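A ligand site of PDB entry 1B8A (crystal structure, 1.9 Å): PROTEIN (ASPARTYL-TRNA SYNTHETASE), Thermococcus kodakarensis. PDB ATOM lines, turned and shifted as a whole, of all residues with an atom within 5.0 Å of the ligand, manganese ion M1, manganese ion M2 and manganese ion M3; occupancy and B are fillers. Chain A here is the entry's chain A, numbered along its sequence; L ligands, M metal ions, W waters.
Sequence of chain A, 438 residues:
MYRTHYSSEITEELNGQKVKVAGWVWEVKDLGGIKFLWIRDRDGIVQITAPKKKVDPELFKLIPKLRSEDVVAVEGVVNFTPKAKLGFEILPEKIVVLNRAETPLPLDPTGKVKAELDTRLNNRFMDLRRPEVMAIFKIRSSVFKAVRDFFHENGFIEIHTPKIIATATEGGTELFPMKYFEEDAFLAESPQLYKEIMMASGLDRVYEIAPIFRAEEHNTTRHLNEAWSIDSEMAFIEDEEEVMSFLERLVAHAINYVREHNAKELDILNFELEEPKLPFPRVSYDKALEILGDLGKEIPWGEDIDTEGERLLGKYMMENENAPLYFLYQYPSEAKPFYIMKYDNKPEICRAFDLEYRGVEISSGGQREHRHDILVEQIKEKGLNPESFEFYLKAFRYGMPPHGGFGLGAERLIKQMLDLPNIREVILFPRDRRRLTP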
ATOM      1  N   GLU A 174      -9.185   0.151 -33.798  1.00  0.00           N
ATOM      2  CA  GLU A 174      -8.449  -0.730 -32.918  1.00  0.00           C
ATOM      3  C   GLU A 174      -8.016  -2.031 -33.569  1.00  0.00           C
ATOM      4  O   GLU A 174      -7.691  -2.986 -32.884  1.00  0.00           O
ATOM      5  CB  GLU A 174      -9.270  -1.002 -31.659  1.00  0.00           C
ATOM      6  CG  GLU A 174      -9.297   0.177 -30.718  1.00  0.00           C
ATOM      7  CD  GLU A 174     -10.113  -0.078 -29.484  1.00  0.00           C
ATOM      8  OE1 GLU A 174     -10.194  -1.256 -29.059  1.00  0.00           O
ATOM      9  OE2 GLU A 174     -10.668   0.898 -28.923  1.00  0.00           O
ATOM     10  N   ILE A 212      -4.347 -12.267 -28.885  1.00  0.00           N
ATOM     11  CA  ILE A 212      -5.346 -11.422 -29.521  1.00  0.00           C
ATOM     12  C   ILE A 212      -4.568 -10.133 -29.767  1.00  0.00           C
ATOM     13  O   ILE A 212      -3.600  -9.860 -29.056  1.00  0.00           O
ATOM     14  CB  ILE A 212      -6.588 -11.143 -28.661  1.00  0.00           C
ATOM     15  CG1 ILE A 212      -6.190 -10.614 -27.294  1.00  0.00           C
ATOM     16  CG2 ILE A 212      -7.446 -12.421 -28.597  1.00  0.00           C
ATOM     17  CD1 ILE A 212      -7.388 -10.001 -26.534  1.00  0.00           C
ATOM     18  N   ARG A 214      -4.896  -5.871 -30.609  1.00  0.00           N
ATOM     19  CA  ARG A 214      -5.757  -4.707 -30.693  1.00  0.00           C
ATOM     20  C   ARG A 214      -4.907  -3.457 -30.741  1.00  0.00           C
ATOM     21  O   ARG A 214      -4.016  -3.298 -29.922  1.00  0.00           O
ATOM     22  CB  ARG A 214      -6.687  -4.684 -29.476  1.00  0.00           C
ATOM     23  CG  ARG A 214      -7.521  -5.973 -29.329  1.00  0.00           C
ATOM     24  CD  ARG A 214      -8.659  -5.827 -28.344  1.00  0.00           C
ATOM     25  NE  ARG A 214      -9.417  -7.060 -28.183  1.00  0.00           N
ATOM     26  CZ  ARG A 214     -10.628  -7.117 -27.661  1.00  0.00           C
ATOM     27  NH1 ARG A 214     -11.220  -5.989 -27.256  1.00  0.00           N
ATOM     28  NH2 ARG A 214     -11.257  -8.274 -27.542  1.00  0.00           N
ATOM     29  N   GLU A 216      -4.798  -0.398 -29.646  1.00  0.00           N
ATOM     30  CA  GLU A 216      -5.441   0.490 -28.689  1.00  0.00           C
ATOM     31  C   GLU A 216      -5.077   1.933 -28.968  1.00  0.00           C
ATOM     32  O   GLU A 216      -3.920   2.251 -29.277  1.00  0.00           O
ATOM     33  CB  GLU A 216      -5.054   0.114 -27.241  1.00  0.00           C
ATOM     34  CG  GLU A 216      -5.519  -1.294 -26.761  1.00  0.00           C
ATOM     35  CD  GLU A 216      -7.039  -1.411 -26.604  1.00  0.00           C
ATOM     36  OE1 GLU A 216      -7.694  -0.372 -26.392  1.00  0.00           O
ATOM     37  OE2 GLU A 216      -7.571  -2.542 -26.661  1.00  0.00           O
ATOM     38  N   ARG A 222      -3.683  -0.764 -17.971  1.00  0.00           N
ATOM     39  CA  ARG A 222      -4.486  -1.986 -18.026  1.00  0.00           C
ATOM     40  C   ARG A 222      -4.704  -2.573 -19.419  1.00  0.00           C
ATOM     41  O   ARG A 222      -5.430  -3.574 -19.547  1.00  0.00           O
ATOM     42  CB  ARG A 222      -5.850  -1.777 -17.357  1.00  0.00           C
ATOM     43  CG  ARG A 222      -6.791  -0.962 -18.226  1.00  0.00           C
ATOM     44  CD  ARG A 222      -8.282  -1.386 -18.140  1.00  0.00           C
ATOM     45  NE  ARG A 222      -8.989  -0.925 -16.945  1.00  0.00           N
ATOM     46  CZ  ARG A 222     -10.305  -1.092 -16.747  1.00  0.00           C
ATOM     47  NH1 ARG A 222     -11.072  -1.716 -17.645  1.00  0.00           N
ATOM     48  NH2 ARG A 222     -10.865  -0.626 -15.636  1.00  0.00           N
ATOM     49  N   HIS A 223      -4.114  -1.962 -20.452  1.00  0.00           N
ATOM     50  CA  HIS A 223      -4.250  -2.475 -21.824  1.00  0.00           C
ATOM     51  C   HIS A 223      -2.910  -2.718 -22.500  1.00  0.00           C
ATOM     52  O   HIS A 223      -1.926  -2.024 -22.218  1.00  0.00           O
ATOM     53  CB  HIS A 223      -5.003  -1.500 -22.734  1.00  0.00           C
ATOM     54  CG  HIS A 223      -6.431  -1.295 -22.376  1.00  0.00           C
ATOM     55  ND1 HIS A 223      -6.838  -0.488 -21.341  1.00  0.00           N
ATOM     56  CD2 HIS A 223      -7.572  -1.727 -22.990  1.00  0.00           C
ATOM     57  CE1 HIS A 223      -8.163  -0.431 -21.323  1.00  0.00           C
ATOM     58  NE2 HIS A 223      -8.627  -1.174 -22.318  1.00  0.00           N
ATOM     59  N   LEU A 224      -2.872  -3.705 -23.395  1.00  0.00           N
ATOM     60  CA  LEU A 224      -1.666  -3.992 -24.198  1.00  0.00           C
ATOM     61  C   LEU A 224      -2.179  -4.102 -25.631  1.00  0.00           C
ATOM     62  O   LEU A 224      -3.378  -4.253 -25.835  1.00  0.00           O
ATOM     63  CB  LEU A 224      -1.059  -5.333 -23.809  1.00  0.00           C
ATOM     64  CG  LEU A 224      -0.524  -5.392 -22.390  1.00  0.00           C
ATOM     65  CD1 LEU A 224      -0.402  -6.867 -21.932  1.00  0.00           C
ATOM     66  CD2 LEU A 224       0.780  -4.675 -22.334  1.00  0.00           C
ATOM     67  N   ALA A 227      -2.188  -9.490 -26.415  1.00  0.00           N
ATOM     68  CA  ALA A 227      -2.494 -10.113 -25.131  1.00  0.00           C
ATOM     69  C   ALA A 227      -2.878 -11.544 -25.358  1.00  0.00           C
ATOM     70  O   ALA A 227      -2.998 -11.975 -26.515  1.00  0.00           O
ATOM     71  CB  ALA A 227      -3.678  -9.371 -24.444  1.00  0.00           C
ATOM     72  N   SER A 229      -5.835 -14.264 -24.622  1.00  0.00           N
ATOM     73  CA  SER A 229      -7.219 -14.365 -24.214  1.00  0.00           C
ATOM     74  C   SER A 229      -7.611 -15.814 -23.992  1.00  0.00           C
ATOM     75  O   SER A 229      -7.236 -16.703 -24.780  1.00  0.00           O
ATOM     76  CB  SER A 229      -8.135 -13.727 -25.275  1.00  0.00           C
ATOM     77  OG  SER A 229      -9.493 -13.881 -24.910  1.00  0.00           O
ATOM     78  N   LYS A 336     -23.624  -3.186 -25.910  1.00  0.00           N
ATOM     79  CA  LYS A 336     -22.937  -4.459 -26.146  1.00  0.00           C
ATOM     80  C   LYS A 336     -23.031  -4.892 -27.604  1.00  0.00           C
ATOM     81  O   LYS A 336     -23.844  -4.348 -28.360  1.00  0.00           O
ATOM     82  CB  LYS A 336     -23.530  -5.521 -25.206  1.00  0.00           C
ATOM     83  CG  LYS A 336     -23.181  -5.292 -23.749  1.00  0.00           C
ATOM     84  CD  LYS A 336     -21.695  -5.539 -23.454  1.00  0.00           C
ATOM     85  CE  LYS A 336     -21.400  -5.400 -21.954  1.00  0.00           C
ATOM     86  NZ  LYS A 336     -19.989  -5.828 -21.607  1.00  0.00           N
ATOM     87  N   ASP A 354     -19.943  -8.683 -17.289  1.00  0.00           N
ATOM     88  CA  ASP A 354     -18.517  -8.393 -17.132  1.00  0.00           C
ATOM     89  C   ASP A 354     -18.136  -8.923 -15.761  1.00  0.00           C
ATOM     90  O   ASP A 354     -18.933  -8.793 -14.817  1.00  0.00           O
ATOM     91  CB  ASP A 354     -18.234  -6.886 -17.108  1.00  0.00           C
ATOM     92  CG  ASP A 354     -18.034  -6.272 -18.490  1.00  0.00           C
ATOM     93  OD1 ASP A 354     -18.421  -6.867 -19.518  1.00  0.00           O
ATOM     94  OD2 ASP A 354     -17.491  -5.153 -18.544  1.00  0.00           O
ATOM     95  N   GLU A 361     -12.216  -4.773 -15.035  1.00  0.00           N
ATOM     96  CA  GLU A 361     -12.764  -5.840 -15.836  1.00  0.00           C
ATOM     97  C   GLU A 361     -11.696  -6.869 -16.196  1.00  0.00           C
ATOM     98  O   GLU A 361     -10.591  -6.490 -16.639  1.00  0.00           O
ATOM     99  CB  GLU A 361     -13.294  -5.283 -17.143  1.00  0.00           C
ATOM    100  CG  GLU A 361     -13.915  -6.348 -18.026  1.00  0.00           C
ATOM    101  CD  GLU A 361     -14.198  -5.783 -19.372  1.00  0.00           C
ATOM    102  OE1 GLU A 361     -14.480  -4.571 -19.415  1.00  0.00           O
ATOM    103  OE2 GLU A 361     -14.153  -6.517 -20.365  1.00  0.00           O
ATOM    104  N   ILE A 362     -12.007  -8.147 -15.990  1.00  0.00           N
ATOM    105  CA  ILE A 362     -11.072  -9.181 -16.370  1.00  0.00           C
ATOM    106  C   ILE A 362     -11.723 -10.061 -17.458  1.00  0.00           C
ATOM    107  O   ILE A 362     -11.032 -10.780 -18.184  1.00  0.00           O
ATOM    108  CB  ILE A 362     -10.607 -10.084 -15.176  1.00  0.00           C
ATOM    109  CG1 ILE A 362     -11.779 -10.751 -14.480  1.00  0.00           C
ATOM    110  CG2 ILE A 362      -9.807  -9.231 -14.152  1.00  0.00           C
ATOM    111  CD1 ILE A 362     -11.297 -11.840 -13.498  1.00  0.00           C
ATOM    112  N   SER A 363     -13.044  -9.981 -17.584  1.00  0.00           N
ATOM    113  CA  SER A 363     -13.733 -10.795 -18.582  1.00  0.00           C
ATOM    114  C   SER A 363     -15.087 -10.222 -18.975  1.00  0.00           C
ATOM    115  O   SER A 363     -15.700  -9.531 -18.181  1.00  0.00           O
ATOM    116  CB  SER A 363     -13.937 -12.230 -18.032  1.00  0.00           C
ATOM    117  OG  SER A 363     -14.580 -13.073 -19.001  1.00  0.00           O
ATOM    118  N   SER A 364     -15.534 -10.536 -20.199  1.00  0.00           N
ATOM    119  CA  SER A 364     -16.842 -10.154 -20.732  1.00  0.00           C
ATOM    120  C   SER A 364     -17.397 -11.379 -21.417  1.00  0.00           C
ATOM    121  O   SER A 364     -16.644 -12.181 -21.967  1.00  0.00           O
ATOM    122  CB  SER A 364     -16.756  -9.042 -21.797  1.00  0.00           C
ATOM    123  OG  SER A 364     -16.918  -7.799 -21.171  1.00  0.00           O
ATOM    124  N   GLY A 407     -14.760 -14.034 -22.888  1.00  0.00           N
ATOM    125  CA  GLY A 407     -13.366 -13.812 -23.209  1.00  0.00           C
ATOM    126  C   GLY A 407     -12.776 -13.358 -21.861  1.00  0.00           C
ATOM    127  O   GLY A 407     -13.238 -12.382 -21.299  1.00  0.00           O
ATOM    128  N   LEU A 408     -11.784 -14.082 -21.344  1.00  0.00           N
ATOM    129  CA  LEU A 408     -11.124 -13.786 -20.065  1.00  0.00           C
ATOM    130  C   LEU A 408      -9.646 -13.432 -20.359  1.00  0.00           C
ATOM    131  O   LEU A 408      -8.903 -14.267 -20.860  1.00  0.00           O
ATOM    132  CB  LEU A 408     -11.213 -15.046 -19.173  1.00  0.00           C
ATOM    133  CG  LEU A 408     -10.327 -15.159 -17.932  1.00  0.00           C
ATOM    134  CD1 LEU A 408     -10.644 -14.026 -16.973  1.00  0.00           C
ATOM    135  CD2 LEU A 408     -10.501 -16.535 -17.263  1.00  0.00           C
ATOM    136  N   GLY A 409      -9.245 -12.181 -20.079  1.00  0.00           N
ATOM    137  CA  GLY A 409      -7.873 -11.761 -20.352  1.00  0.00           C
ATOM    138  C   GLY A 409      -6.900 -12.396 -19.385  1.00  0.00           C
ATOM    139  O   GLY A 409      -7.042 -12.255 -18.171  1.00  0.00           O
ATOM    140  N   ARG A 412      -5.004  -9.691 -17.714  1.00  0.00           N
ATOM    141  CA  ARG A 412      -5.901  -8.998 -16.797  1.00  0.00           C
ATOM    142  C   ARG A 412      -6.109  -9.807 -15.534  1.00  0.00           C
ATOM    143  O   ARG A 412      -6.080  -9.261 -14.431  1.00  0.00           O
ATOM    144  CB  ARG A 412      -7.254  -8.749 -17.464  1.00  0.00           C
ATOM    145  CG  ARG A 412      -7.267  -7.581 -18.409  1.00  0.00           C
ATOM    146  CD  ARG A 412      -7.419  -6.233 -17.649  1.00  0.00           C
ATOM    147  NE  ARG A 412      -7.395  -5.168 -18.632  1.00  0.00           N
ATOM    148  CZ  ARG A 412      -8.453  -4.715 -19.294  1.00  0.00           C
ATOM    149  NH1 ARG A 412      -9.657  -5.215 -19.076  1.00  0.00           N
ATOM    150  NH2 ARG A 412      -8.272  -3.839 -20.273  1.00  0.00           N
ATOM    151  N   ILE A 423      -0.107  -3.692 -16.040  1.00  0.00           N
ATOM    152  CA  ILE A 423      -0.273  -4.936 -16.777  1.00  0.00           C
ATOM    153  C   ILE A 423       1.048  -5.384 -17.456  1.00  0.00           C
ATOM    154  O   ILE A 423       1.236  -6.576 -17.738  1.00  0.00           O
ATOM    155  CB  ILE A 423      -1.442  -4.784 -17.788  1.00  0.00           C
ATOM    156  CG1 ILE A 423      -1.903  -6.170 -18.259  1.00  0.00           C
ATOM    157  CG2 ILE A 423      -1.028  -3.879 -18.932  1.00  0.00           C
ATOM    158  CD1 ILE A 423      -3.208  -6.111 -19.066  1.00  0.00           C
HETATM  159  P1  LIG L   1     -11.760  -2.798 -21.675  1.00  0.00           P
HETATM  160  O1  LIG L   1     -10.753  -3.014 -20.578  1.00  0.00           O
HETATM  161  O2  LIG L   1     -13.046  -2.096 -21.364  1.00  0.00           O
HETATM  162  O3  LIG L   1     -11.006  -1.953 -22.784  1.00  0.00           O
HETATM  163  P2  LIG L   1     -13.105  -4.518 -23.585  1.00  0.00           P
HETATM  164  O4  LIG L   1     -14.445  -4.438 -22.950  1.00  0.00           O
HETATM  165  O5  LIG L   1     -12.845  -3.767 -24.841  1.00  0.00           O
HETATM  166  O6  LIG L   1     -12.051  -4.165 -22.439  1.00  0.00           O
HETATM  167  P3  LIG L   1     -13.502  -7.211 -24.614  1.00  0.00           P
HETATM  168  O7  LIG L   1     -14.729  -7.568 -23.898  1.00  0.00           O
HETATM  169  O8  LIG L   1     -13.568  -6.807 -26.025  1.00  0.00           O
HETATM  170  O9  LIG L   1     -12.738  -6.041 -23.842  1.00  0.00           O
HETATM  171  O10 LIG L   1     -12.442  -8.381 -24.449  1.00  0.00           O
HETATM  172  C1  LIG L   1     -12.619  -9.442 -23.484  1.00  0.00           C
HETATM  173  C2  LIG L   1     -11.510  -9.391 -22.445  1.00  0.00           C
HETATM  174  O11 LIG L   1     -10.230  -9.337 -23.131  1.00  0.00           O
HETATM  175  C3  LIG L   1     -11.477  -8.178 -21.531  1.00  0.00           C
HETATM  176  O12 LIG L   1     -12.345  -8.458 -20.409  1.00  0.00           O
HETATM  177  C4  LIG L   1     -10.017  -8.162 -21.068  1.00  0.00           C
HETATM  178  O13 LIG L   1      -9.790  -9.084 -20.033  1.00  0.00           O
HETATM  179  C5  LIG L   1      -9.285  -8.623 -22.332  1.00  0.00           C
HETATM  180  N1  LIG L   1      -8.778  -7.495 -23.109  1.00  0.00           N
HETATM  181  C6  LIG L   1      -9.441  -6.697 -24.003  1.00  0.00           C
HETATM  182  N2  LIG L   1      -8.703  -5.729 -24.501  1.00  0.00           N
HETATM  183  C7  LIG L   1      -7.459  -5.926 -23.917  1.00  0.00           C
HETATM  184  C8  LIG L   1      -6.232  -5.243 -24.040  1.00  0.00           C
HETATM  185  N3  LIG L   1      -6.025  -4.224 -24.882  1.00  0.00           N
HETATM  186  N4  LIG L   1      -5.194  -5.660 -23.276  1.00  0.00           N
HETATM  187  C9  LIG L   1      -5.385  -6.726 -22.472  1.00  0.00           C
HETATM  188  N5  LIG L   1      -6.475  -7.467 -22.289  1.00  0.00           N
HETATM  189  C10 LIG L   1      -7.493  -7.004 -23.050  1.00  0.00           C
HETATM  190 MN    MN M   1     -11.477  -2.060 -24.941  1.00  0.00          MN
HETATM  191 MN    MN M   2     -15.736  -5.971 -22.113  1.00  0.00          MN
HETATM  192 MN    MN M   3     -14.992  -3.196 -21.055  1.00  0.00          MN
HETATM  193  O   HOH W   1     -17.764  -5.965 -23.759  1.00  0.00           O
HETATM  194  O   HOH W   2     -13.730  -3.866 -27.918  1.00  0.00           O
HETATM  195  O   HOH W   3     -13.656   0.544 -22.241  1.00  0.00           O
HETATM  196  O   HOH W   4     -12.048  -1.997 -27.125  1.00  0.00           O
HETATM  197  O   HOH W   5     -16.186  -1.803 -22.566  1.00  0.00           O
HETATM  198  O   HOH W   6     -17.104  -4.474 -20.824  1.00  0.00           O
HETATM  199  O   HOH W   7     -10.067  -0.289 -25.303  1.00  0.00           O
HETATM  200  O   HOH W   8     -15.692  -2.224 -25.077  1.00  0.00           O
HETATM  201  O   HOH W   9      -9.785  -3.581 -25.562  1.00  0.00           O
HETATM  202  O   HOH W  10     -15.623  -1.896 -19.048  1.00  0.00           O
HETATM  203  O   HOH W  11      -5.423  -9.715 -20.720  1.00  0.00           O
HETATM  204  O   HOH W  12     -13.062  -0.433 -24.685  1.00  0.00           O
HETATM  205  O   HOH W  13     -10.810 -11.492 -25.209  1.00  0.00           O
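NE2 of His 223 touches manganese ion M1 (3.97 Å).
The nearest printed residue that does not touch manganese ion M1 is Glu 216 (4.3 Å).
NE of Arg 412 lies within hydrogen-bond range of O of Arg 222 (2.7 Å).
The side-chain carboxylate (OD1) of Asp 354 is in salt-bridge range of the side-chain amino group (NZ) of Lys 336.
A ring nitrogen (NE2) of His 223 lies within hydrogen-bond range of the guanidinium group of Arg 412.
The backbone carbonyl oxygen (O) of Glu 361 is in hydrogen-bond range of the guanidinium group (NH1) of Arg 412, 2.9 Å away.
O of Ala 227 sits at hydrogen-bond distance from N of Ile 212 (2.7 Å).
The side-chain hydroxyl of Ser 364 sits close to the side-chain carboxylate of Asp 354 (2.4 Å).
The backbone carbonyl oxygen (O) of Ile 362 is in hydrogen-bond range of the backbone NH (N) of Gly 409 (3.0 Å).
O of Ser 364 lies within hydrogen-bond range of N of Gly 407, 2.8 Å away.
One residue has an atom within 4 Å of manganese ion M3: Glu 361.
Manganese ion M3 is bound by OE1 of Glu 361, at 2.2 Å.
An oxygen (O2) of the ligand is bound to manganese ion M3, at 2.3 Å.
Manganese ion M3 is bound by an oxygen (O4) of the ligand.
Water W5 binds manganese ion M3 (2.4 Å).
Water W10 is bound to manganese ion M3.
Manganese ion M3 is bound by water W6, at 2.5 Å.
Manganese ion M3 has six donor atoms within binding distance.
The guanidinium group (NH2) of Arg 412 is in salt-bridge range of an oxygen (O1) of the ligand, at 2.6 Å.
The side-chain carboxylate (OE2) of Glu 216 is in hydrogen-bond range of a nitrogen (N3) of the ligand, 2.9 Å away.
The guanidinium group (NH1) of Arg 222 lies within salt-bridge range of an oxygen (O1) of the ligand (3.2 Å).
N4 of the ligand sits at hydrogen-bond distance from N of Leu 224.
A ring nitrogen (NE2) of His 223 lies within hydrogen-bond range of an oxygen (O1) of the ligand (3.3 Å).
O of Leu 224 lies within hydrogen-bond range of N3 of the ligand (2.8 Å).
O of Ile 362 lies within hydrogen-bond range of O13 of the ligand, 2.8 Å away.
N of Gly 409 sits at hydrogen-bond distance from O13 of the ligand, at 3.1 Å.
The guanidinium group (NH1) of Arg 214 is in salt-bridge range of an oxygen (O8) of the ligand (2.8 Å).
O12 of the ligand sits close to N of Ser 363.
Water W9 lies within hydrogen-bond range of N2 of the ligand (2.6 Å), OE2 of Glu 216 (2.7 Å) and NH1 of Arg 214 (3.3 Å).
Water W7 lies within hydrogen-bond range of OE1 of Glu 216 and NE2 of His 223.
Water W6 lies within hydrogen-bond range of the side-chain carboxylate of Asp 354 (2.4 Å) and the side-chain amino group of Lys 336 (3.3 Å).
Water W11 bridges N5 of the ligand (2.9 Å) and N of Arg 412 (3.0 Å).
Water W13 bridges the side-chain hydroxyl of Ser 229 (2.7 Å) and an oxygen (O11) of the ligand (3.0 Å).
Manganese ion M1 is bound by an oxygen (O5) of the ligand, an oxygen (O3) of the ligand, water W4, water W12, water W7 and water W9.
CB of Ala 227 touches C9 of the ligand, 3.7 Å away.
Gly 407 touches the ligand (O to C2, 3.6 Å).
Within 4 Å of the ligand: Arg 214, Glu 216, Arg 222, His 223, Leu 224, Ala 227, Glu 361, Ile 362, Ser 363, Ser 364, Gly 407, Gly 409 and Arg 412.
Residues that only touch manganese ion M2: Asp 354.
Within 4 Å of manganese ion M2: Asp 354, Glu 361 and Ser 364.
The nearest printed residue that does not touch manganese ion M2 is Lys 336 (4.3 Å).
Manganese ion M2 is bound by O4 of the ligand (2.2 Å), OG of Ser 364 (2.4 Å), water W6 (2.4 Å), OE2 of Glu 361 (2.4 Å), O7 of the ligand (2.6 Å) and water W1 (2.6 Å).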
